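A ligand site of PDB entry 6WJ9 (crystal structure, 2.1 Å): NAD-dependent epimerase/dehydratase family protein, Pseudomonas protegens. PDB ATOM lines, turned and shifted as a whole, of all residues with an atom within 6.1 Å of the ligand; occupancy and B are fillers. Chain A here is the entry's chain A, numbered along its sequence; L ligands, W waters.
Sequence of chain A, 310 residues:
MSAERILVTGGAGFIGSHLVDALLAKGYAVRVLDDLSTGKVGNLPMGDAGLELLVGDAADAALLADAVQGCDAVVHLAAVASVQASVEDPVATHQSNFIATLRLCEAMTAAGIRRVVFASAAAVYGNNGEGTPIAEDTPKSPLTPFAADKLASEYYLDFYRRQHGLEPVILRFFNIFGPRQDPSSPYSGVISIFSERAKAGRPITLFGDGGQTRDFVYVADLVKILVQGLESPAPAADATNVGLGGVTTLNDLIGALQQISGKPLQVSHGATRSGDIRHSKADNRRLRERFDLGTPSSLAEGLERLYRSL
OD2 of Asp 276 is in hydrogen-bond range of O6 of the ligand, at 2.7 Å. The backbone carbonyl oxygen of Thr 205 sits at hydrogen-bond distance from a nitrogen (N2) of the ligand (2.8 Å). The backbone NH of Phe 207 is in hydrogen-bond range of an oxygen (O2) of the ligand (2.8 Å). N of Val 190 lies within hydrogen-bond range of O9 of the ligand (2.8 Å). An oxygen (O11) of the ligand is in salt-bridge range of the guanidinium group (NE) of Arg 214 (3.0 Å). ND2 of Asn 175 sits at hydrogen-bond distance from O11 of the ligand (3.0 Å). An oxygen (O6) of the ligand lies within hydrogen-bond range of the side-chain amide nitrogen (NE2) of Gln 212. The guanidinium group (NH1) of Arg 273 is in salt-bridge range of an oxygen (O8) of the ligand (3.9 Å).
The side-chain carboxylate (OD1) of Asp 276 is in salt-bridge range of the guanidinium group (NH2) of Arg 214 (3.0 Å). The side-chain carboxylate of Asp 276 is in hydrogen-bond range of the side-chain amide nitrogen of Gln 212 (3.3 Å). O of Phe 207 is in hydrogen-bond range of NE2 of Gln 212, at 2.8 Å. O of Ile 277 lies within hydrogen-bond range of NH2 of Arg 214, at 2.8 Å. The backbone NH (N) of Leu 250 lies within hydrogen-bond range of the backbone carbonyl oxygen (O) of Gln 212 (3.0 Å). The backbone carbonyl oxygen (O) of Pro 186 sits at hydrogen-bond distance from the guanidinium group (NH2) of Arg 273 (2.9 Å).
Gly 189 touches the ligand. Phe 194 touches the ligand. Leu 206 touches the ligand. Leu 250 touches the ligand. Hydrophobic or aromatic side chains within 4 Å of the ligand: Val 190, Phe 194, Leu 206, Phe 207 and Leu 250. Of the 22 residues printed, 12 come within 4 Å of the ligand.
Water W4 bridges NH1 of Arg 273 (2.5 Å) and O8 of the ligand (2.8 Å). Water W8 lies within hydrogen-bond range of the side-chain carboxylate of Asp 276, an oxygen (O4) of the ligand, the backbone carbonyl oxygen of Phe 207, the backbone NH of Arg 273 and the side-chain amide nitrogen of Gln 212. Water W7 lies within hydrogen-bond range of the backbone carbonyl oxygen (O) of Ser 188, an oxygen (O8) of the ligand and the guanidinium group (NH1) of Arg 273. Water W2 lies within hydrogen-bond range of OD1 of Asp 276 (2.6 Å) and O12 of the ligand (2.9 Å). Water W3 lies within hydrogen-bond range of the side-chain amide nitrogen (ND2) of Asn 175 and an oxygen (O9) of the ligand. Water W5 bridges N of Thr 205 and O3 of the ligand.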
ATOM      1  N   VAL A  83      -4.938  -8.099   7.911  1.00  0.00           N
ATOM      2  CA  VAL A  83      -6.056  -7.311   7.406  1.00  0.00           C
ATOM      3  C   VAL A  83      -7.371  -7.869   7.941  1.00  0.00           C
ATOM      4  O   VAL A  83      -8.276  -7.108   8.341  1.00  0.00           O
ATOM      5  CB  VAL A  83      -6.030  -7.290   5.871  1.00  0.00           C
ATOM      6  CG1 VAL A  83      -7.287  -6.615   5.333  1.00  0.00           C
ATOM      7  CG2 VAL A  83      -4.776  -6.555   5.381  1.00  0.00           C
ATOM      8  N   ASN A 175       4.590  -7.671  -1.257  1.00  0.00           N
ATOM      9  CA  ASN A 175       4.445  -8.973  -0.577  1.00  0.00           C
ATOM     10  C   ASN A 175       5.790  -9.439  -0.004  1.00  0.00           C
ATOM     11  O   ASN A 175       6.605 -10.040  -0.713  1.00  0.00           O
ATOM     12  CB  ASN A 175       3.849 -10.014  -1.516  1.00  0.00           C
ATOM     13  CG  ASN A 175       2.387  -9.697  -1.860  1.00  0.00           C
ATOM     14  OD1 ASN A 175       2.109  -8.787  -2.639  1.00  0.00           O
ATOM     15  ND2 ASN A 175       1.462 -10.444  -1.278  1.00  0.00           N
ATOM     16  N   PRO A 186      -4.678 -18.835   8.491  1.00  0.00           N
ATOM     17  CA  PRO A 186      -5.046 -19.092   7.094  1.00  0.00           C
ATOM     18  C   PRO A 186      -4.770 -17.915   6.175  1.00  0.00           C
ATOM     19  O   PRO A 186      -4.574 -18.101   4.974  1.00  0.00           O
ATOM     20  CB  PRO A 186      -6.546 -19.400   7.173  1.00  0.00           C
ATOM     21  CG  PRO A 186      -7.001 -18.679   8.398  1.00  0.00           C
ATOM     22  CD  PRO A 186      -5.866 -18.791   9.373  1.00  0.00           C
ATOM     23  N   TYR A 187      -4.743 -16.700   6.716  1.00  0.00           N
ATOM     24  CA  TYR A 187      -4.448 -15.503   5.957  1.00  0.00           C
ATOM     25  C   TYR A 187      -2.982 -15.092   6.057  1.00  0.00           C
ATOM     26  O   TYR A 187      -2.630 -13.983   5.660  1.00  0.00           O
ATOM     27  CB  TYR A 187      -5.348 -14.350   6.411  1.00  0.00           C
ATOM     28  CG  TYR A 187      -6.814 -14.680   6.357  1.00  0.00           C
ATOM     29  CD1 TYR A 187      -7.500 -14.729   5.144  1.00  0.00           C
ATOM     30  CD2 TYR A 187      -7.531 -14.970   7.518  1.00  0.00           C
ATOM     31  CE1 TYR A 187      -8.841 -15.036   5.091  1.00  0.00           C
ATOM     32  CE2 TYR A 187      -8.875 -15.280   7.474  1.00  0.00           C
ATOM     33  CZ  TYR A 187      -9.529 -15.311   6.256  1.00  0.00           C
ATOM     34  OH  TYR A 187     -10.862 -15.629   6.212  1.00  0.00           O
ATOM     35  N   SER A 188      -2.125 -15.968   6.605  1.00  0.00           N
ATOM     36  CA  SER A 188      -0.698 -15.733   6.541  1.00  0.00           C
ATOM     37  C   SER A 188      -0.245 -15.677   5.080  1.00  0.00           C
ATOM     38  O   SER A 188      -0.939 -16.133   4.177  1.00  0.00           O
ATOM     39  CB  SER A 188       0.066 -16.843   7.267  1.00  0.00           C
ATOM     40  OG  SER A 188      -0.410 -16.972   8.590  1.00  0.00           O
ATOM     41  N   GLY A 189       0.920 -15.081   4.865  1.00  0.00           N
ATOM     42  CA  GLY A 189       1.458 -14.975   3.517  1.00  0.00           C
ATOM     43  C   GLY A 189       1.504 -16.323   2.818  1.00  0.00           C
ATOM     44  O   GLY A 189       1.763 -17.347   3.454  1.00  0.00           O
ATOM     45  N   VAL A 190       1.215 -16.338   1.512  1.00  0.00           N
ATOM     46  CA  VAL A 190       1.091 -17.606   0.797  1.00  0.00           C
ATOM     47  C   VAL A 190       2.416 -18.350   0.786  1.00  0.00           C
ATOM     48  O   VAL A 190       2.445 -19.591   0.824  1.00  0.00           O
ATOM     49  CB  VAL A 190       0.546 -17.369  -0.625  1.00  0.00           C
ATOM     50  CG1 VAL A 190       1.517 -16.507  -1.437  1.00  0.00           C
ATOM     51  CG2 VAL A 190       0.272 -18.695  -1.319  1.00  0.00           C
ATOM     52  N   ILE A 191       3.530 -17.616   0.760  1.00  0.00           N
ATOM     53  CA  ILE A 191       4.826 -18.270   0.722  1.00  0.00           C
ATOM     54  C   ILE A 191       5.110 -18.965   2.043  1.00  0.00           C
ATOM     55  O   ILE A 191       5.568 -20.107   2.069  1.00  0.00           O
ATOM     56  CB  ILE A 191       5.927 -17.261   0.347  1.00  0.00           C
ATOM     57  CG1 ILE A 191       5.816 -16.895  -1.139  1.00  0.00           C
ATOM     58  CG2 ILE A 191       7.322 -17.852   0.635  1.00  0.00           C
ATOM     59  CD1 ILE A 191       6.865 -15.906  -1.605  1.00  0.00           C
ATOM     60  N   ILE A 193       2.943 -20.188   4.048  1.00  0.00           N
ATOM     61  CA  ILE A 193       2.076 -21.360   4.131  1.00  0.00           C
ATOM     62  C   ILE A 193       2.561 -22.461   3.193  1.00  0.00           C
ATOM     63  O   ILE A 193       2.694 -23.621   3.600  1.00  0.00           O
ATOM     64  CB  ILE A 193       0.617 -20.994   3.831  1.00  0.00           C
ATOM     65  CG1 ILE A 193       0.091 -19.985   4.853  1.00  0.00           C
ATOM     66  CG2 ILE A 193      -0.256 -22.264   3.827  1.00  0.00           C
ATOM     67  CD1 ILE A 193      -1.330 -19.498   4.570  1.00  0.00           C
ATOM     68  N   PHE A 194       2.821 -22.115   1.932  1.00  0.00           N
ATOM     69  CA  PHE A 194       3.261 -23.134   0.982  1.00  0.00           C
ATOM     70  C   PHE A 194       4.574 -23.757   1.434  1.00  0.00           C
ATOM     71  O   PHE A 194       4.762 -24.982   1.335  1.00  0.00           O
ATOM     72  CB  PHE A 194       3.383 -22.556  -0.426  1.00  0.00           C
ATOM     73  CG  PHE A 194       2.064 -22.391  -1.140  1.00  0.00           C
ATOM     74  CD1 PHE A 194       0.871 -22.663  -0.493  1.00  0.00           C
ATOM     75  CD2 PHE A 194       2.020 -21.965  -2.458  1.00  0.00           C
ATOM     76  CE1 PHE A 194      -0.341 -22.509  -1.147  1.00  0.00           C
ATOM     77  CE2 PHE A 194       0.813 -21.817  -3.123  1.00  0.00           C
ATOM     78  CZ  PHE A 194      -0.373 -22.091  -2.465  1.00  0.00           C
ATOM     79  N   THR A 205      -3.345 -25.901  -0.469  1.00  0.00           N
ATOM     80  CA  THR A 205      -4.584 -25.562  -1.143  1.00  0.00           C
ATOM     81  C   THR A 205      -4.329 -24.320  -1.984  1.00  0.00           C
ATOM     82  O   THR A 205      -3.944 -23.277  -1.466  1.00  0.00           O
ATOM     83  CB  THR A 205      -5.709 -25.319  -0.148  1.00  0.00           C
ATOM     84  OG1 THR A 205      -5.979 -26.529   0.568  1.00  0.00           O
ATOM     85  CG2 THR A 205      -6.967 -24.862  -0.889  1.00  0.00           C
ATOM     86  N   LEU A 206      -4.535 -24.448  -3.291  1.00  0.00           N
ATOM     87  CA  LEU A 206      -4.434 -23.338  -4.211  1.00  0.00           C
ATOM     88  C   LEU A 206      -5.831 -22.776  -4.422  1.00  0.00           C
ATOM     89  O   LEU A 206      -6.734 -23.486  -4.885  1.00  0.00           O
ATOM     90  CB  LEU A 206      -3.818 -23.797  -5.537  1.00  0.00           C
ATOM     91  CG  LEU A 206      -3.627 -22.773  -6.647  1.00  0.00           C
ATOM     92  CD1 LEU A 206      -2.612 -21.703  -6.223  1.00  0.00           C
ATOM     93  CD2 LEU A 206      -3.210 -23.474  -7.920  1.00  0.00           C
ATOM     94  N   PHE A 207      -6.010 -21.499  -4.073  1.00  0.00           N
ATOM     95  CA  PHE A 207      -7.286 -20.801  -4.235  1.00  0.00           C
ATOM     96  C   PHE A 207      -7.325 -20.156  -5.617  1.00  0.00           C
ATOM     97  O   PHE A 207      -6.759 -19.085  -5.821  1.00  0.00           O
ATOM     98  CB  PHE A 207      -7.471 -19.765  -3.135  1.00  0.00           C
ATOM     99  CG  PHE A 207      -7.602 -20.355  -1.758  1.00  0.00           C
ATOM    100  CD1 PHE A 207      -8.598 -21.257  -1.475  1.00  0.00           C
ATOM    101  CD2 PHE A 207      -6.726 -19.989  -0.749  1.00  0.00           C
ATOM    102  CE1 PHE A 207      -8.719 -21.807  -0.202  1.00  0.00           C
ATOM    103  CE2 PHE A 207      -6.840 -20.529   0.530  1.00  0.00           C
ATOM    104  CZ  PHE A 207      -7.838 -21.446   0.794  1.00  0.00           C
ATOM    105  N   GLY A 208      -7.991 -20.808  -6.560  1.00  0.00           N
ATOM    106  CA  GLY A 208      -8.007 -20.355  -7.937  1.00  0.00           C
ATOM    107  C   GLY A 208      -7.126 -21.204  -8.821  1.00  0.00           C
ATOM    108  O   GLY A 208      -6.740 -22.333  -8.484  1.00  0.00           O
ATOM    109  N   GLN A 212      -2.572 -16.131 -10.593  1.00  0.00           N
ATOM    110  CA  GLN A 212      -2.371 -14.878  -9.884  1.00  0.00           C
ATOM    111  C   GLN A 212      -0.876 -14.571  -9.752  1.00  0.00           C
ATOM    112  O   GLN A 212      -0.065 -15.474  -9.542  1.00  0.00           O
ATOM    113  CB  GLN A 212      -2.991 -14.930  -8.493  1.00  0.00           C
ATOM    114  CG  GLN A 212      -4.433 -15.360  -8.436  1.00  0.00           C
ATOM    115  CD  GLN A 212      -4.572 -16.800  -7.969  1.00  0.00           C
ATOM    116  OE1 GLN A 212      -4.144 -17.725  -8.647  1.00  0.00           O
ATOM    117  NE2 GLN A 212      -5.174 -16.985  -6.797  1.00  0.00           N
ATOM    118  N   ARG A 214       2.178 -11.961  -7.921  1.00  0.00           N
ATOM    119  CA  ARG A 214       2.503 -11.049  -6.835  1.00  0.00           C
ATOM    120  C   ARG A 214       3.945 -10.580  -6.998  1.00  0.00           C
ATOM    121  O   ARG A 214       4.776 -11.256  -7.610  1.00  0.00           O
ATOM    122  CB  ARG A 214       2.322 -11.703  -5.454  1.00  0.00           C
ATOM    123  CG  ARG A 214       0.892 -12.079  -5.124  1.00  0.00           C
ATOM    124  CD  ARG A 214       0.061 -10.827  -4.967  1.00  0.00           C
ATOM    125  NE  ARG A 214      -1.283 -11.106  -4.470  1.00  0.00           N
ATOM    126  CZ  ARG A 214      -2.321 -11.386  -5.265  1.00  0.00           C
ATOM    127  NH1 ARG A 214      -2.151 -11.427  -6.581  1.00  0.00           N
ATOM    128  NH2 ARG A 214      -3.522 -11.606  -4.735  1.00  0.00           N
ATOM    129  N   PHE A 216       6.828 -10.287  -5.011  1.00  0.00           N
ATOM    130  CA  PHE A 216       7.370 -10.791  -3.748  1.00  0.00           C
ATOM    131  C   PHE A 216       8.724 -10.160  -3.453  1.00  0.00           C
ATOM    132  O   PHE A 216       9.574 -10.030  -4.339  1.00  0.00           O
ATOM    133  CB  PHE A 216       7.546 -12.316  -3.774  1.00  0.00           C
ATOM    134  CG  PHE A 216       6.261 -13.086  -3.859  1.00  0.00           C
ATOM    135  CD1 PHE A 216       5.312 -13.022  -2.843  1.00  0.00           C
ATOM    136  CD2 PHE A 216       6.008 -13.915  -4.957  1.00  0.00           C
ATOM    137  CE1 PHE A 216       4.133 -13.746  -2.910  1.00  0.00           C
ATOM    138  CE2 PHE A 216       4.831 -14.648  -5.028  1.00  0.00           C
ATOM    139  CZ  PHE A 216       3.888 -14.552  -4.007  1.00  0.00           C
ATOM    140  N   LEU A 250       1.492 -17.951  -8.797  1.00  0.00           N
ATOM    141  CA  LEU A 250       1.440 -18.976  -7.758  1.00  0.00           C
ATOM    142  C   LEU A 250       1.880 -20.324  -8.307  1.00  0.00           C
ATOM    143  O   LEU A 250       2.564 -21.094  -7.608  1.00  0.00           O
ATOM    144  CB  LEU A 250       0.032 -19.060  -7.176  1.00  0.00           C
ATOM    145  CG  LEU A 250      -0.478 -17.810  -6.453  1.00  0.00           C
ATOM    146  CD1 LEU A 250      -1.839 -18.093  -5.805  1.00  0.00           C
ATOM    147  CD2 LEU A 250       0.532 -17.350  -5.422  1.00  0.00           C
ATOM    148  N   ARG A 273     -10.365 -16.745  -3.947  1.00  0.00           N
ATOM    149  CA  ARG A 273     -10.770 -15.943  -2.797  1.00  0.00           C
ATOM    150  C   ARG A 273     -11.591 -14.741  -3.242  1.00  0.00           C
ATOM    151  O   ARG A 273     -11.257 -14.072  -4.223  1.00  0.00           O
ATOM    152  CB  ARG A 273      -9.546 -15.475  -2.002  1.00  0.00           C
ATOM    153  CG  ARG A 273      -9.169 -16.394  -0.849  1.00  0.00           C
ATOM    154  CD  ARG A 273      -8.006 -15.843  -0.016  1.00  0.00           C
ATOM    155  NE  ARG A 273      -7.703 -16.741   1.102  1.00  0.00           N
ATOM    156  CZ  ARG A 273      -6.583 -16.689   1.826  1.00  0.00           C
ATOM    157  NH1 ARG A 273      -5.642 -15.790   1.549  1.00  0.00           N
ATOM    158  NH2 ARG A 273      -6.397 -17.551   2.811  1.00  0.00           N
ATOM    159  N   ASP A 276     -10.102 -11.242  -4.311  1.00  0.00           N
ATOM    160  CA  ASP A 276      -8.696 -11.437  -4.630  1.00  0.00           C
ATOM    161  C   ASP A 276      -8.292 -10.564  -5.808  1.00  0.00           C
ATOM    162  O   ASP A 276      -9.026 -10.427  -6.787  1.00  0.00           O
ATOM    163  CB  ASP A 276      -8.456 -12.916  -4.956  1.00  0.00           C
ATOM    164  CG  ASP A 276      -7.011 -13.317  -4.866  1.00  0.00           C
ATOM    165  OD1 ASP A 276      -6.238 -12.634  -4.159  1.00  0.00           O
ATOM    166  OD2 ASP A 276      -6.639 -14.318  -5.514  1.00  0.00           O
ATOM    167  N   ILE A 277      -7.120  -9.945  -5.696  1.00  0.00           N
ATOM    168  CA  ILE A 277      -6.500  -9.279  -6.841  1.00  0.00           C
ATOM    169  C   ILE A 277      -5.738 -10.323  -7.639  1.00  0.00           C
ATOM    170  O   ILE A 277      -4.892 -11.038  -7.093  1.00  0.00           O
ATOM    171  CB  ILE A 277      -5.557  -8.153  -6.370  1.00  0.00           C
ATOM    172  CG1 ILE A 277      -6.345  -7.035  -5.672  1.00  0.00           C
ATOM    173  CG2 ILE A 277      -4.777  -7.602  -7.560  1.00  0.00           C
ATOM    174  CD1 ILE A 277      -5.456  -5.974  -5.020  1.00  0.00           C
ATOM    175  N   SER A 280      -0.831  -8.244  -9.284  1.00  0.00           N
ATOM    176  CA  SER A 280      -0.329  -7.184  -8.420  1.00  0.00           C
ATOM    177  C   SER A 280       1.172  -7.023  -8.628  1.00  0.00           C
ATOM    178  O   SER A 280       1.937  -7.954  -8.366  1.00  0.00           O
ATOM    179  CB  SER A 280      -0.619  -7.471  -6.951  1.00  0.00           C
ATOM    180  OG  SER A 280       0.091  -6.533  -6.145  1.00  0.00           O
HETATM  181  C1  LIG L   1      -2.148  -9.067   0.864  1.00  0.00           C
HETATM  182  O1  LIG L   1      -2.852 -10.157   0.333  1.00  0.00           O
HETATM  183  N1  LIG L   1      -3.384 -18.292  -1.522  1.00  0.00           N
HETATM  184  C2  LIG L   1      -3.584 -19.672  -1.880  1.00  0.00           C
HETATM  185  N2  LIG L   1      -3.490 -20.597  -0.858  1.00  0.00           N
HETATM  186  C3  LIG L   1      -3.216 -20.248   0.382  1.00  0.00           C
HETATM  187  C4  LIG L   1      -2.995 -18.819   0.732  1.00  0.00           C
HETATM  188  C5  LIG L   1      -3.086 -17.878  -0.271  1.00  0.00           C
HETATM  189  O2  LIG L   1      -3.851 -20.038  -3.012  1.00  0.00           O
HETATM  190  O3  LIG L   1      -3.129 -21.108   1.249  1.00  0.00           O
HETATM  191  C6  LIG L   1      -3.463 -17.276  -2.546  1.00  0.00           C
HETATM  192  C7  LIG L   1      -4.335 -16.144  -2.171  1.00  0.00           C
HETATM  193  O4  LIG L   1      -5.679 -16.412  -2.388  1.00  0.00           O
HETATM  194  C8  LIG L   1      -3.826 -15.081  -3.069  1.00  0.00           C
HETATM  195  C9  LIG L   1      -2.365 -15.351  -3.122  1.00  0.00           C
HETATM  196  O5  LIG L   1      -2.203 -16.706  -2.789  1.00  0.00           O
HETATM  197  O6  LIG L   1      -4.335 -15.211  -4.354  1.00  0.00           O
HETATM  198  C10 LIG L   1      -1.575 -14.416  -2.237  1.00  0.00           C
HETATM  199  O7  LIG L   1      -2.162 -14.397  -0.964  1.00  0.00           O
HETATM  200  P1  LIG L   1      -1.531 -13.505   0.193  1.00  0.00           P
HETATM  201  O8  LIG L   1      -2.502 -13.474   1.347  1.00  0.00           O
HETATM  202  O9  LIG L   1      -0.194 -14.070   0.587  1.00  0.00           O
HETATM  203  O10 LIG L   1      -1.309 -12.025  -0.311  1.00  0.00           O
HETATM  204  P2  LIG L   1      -2.292 -10.939  -0.909  1.00  0.00           P
HETATM  205  O11 LIG L   1      -1.486  -9.955  -1.730  1.00  0.00           O
HETATM  206  O12 LIG L   1      -3.363 -11.602  -1.740  1.00  0.00           O
HETATM  207  O   HOH W   1      -2.757  -7.927  -3.053  1.00  0.00           O
HETATM  208  O   HOH W   2      -6.105 -12.428  -1.616  1.00  0.00           O
HETATM  209  O   HOH W   3       2.244 -12.400   0.717  1.00  0.00           O
HETATM  210  O   HOH W   4      -5.114 -13.607   0.463  1.00  0.00           O
HETATM  211  O   HOH W   5      -2.558 -24.141   1.301  1.00  0.00           O
HETATM  212  O   HOH W   6      -5.208  -9.464  -3.107  1.00  0.00           O
HETATM  213  O   HOH W   7      -2.911 -16.008   2.568  1.00  0.00           O
HETATM  214  O   HOH W   8      -7.402 -16.501  -4.644  1.00  0.00           O
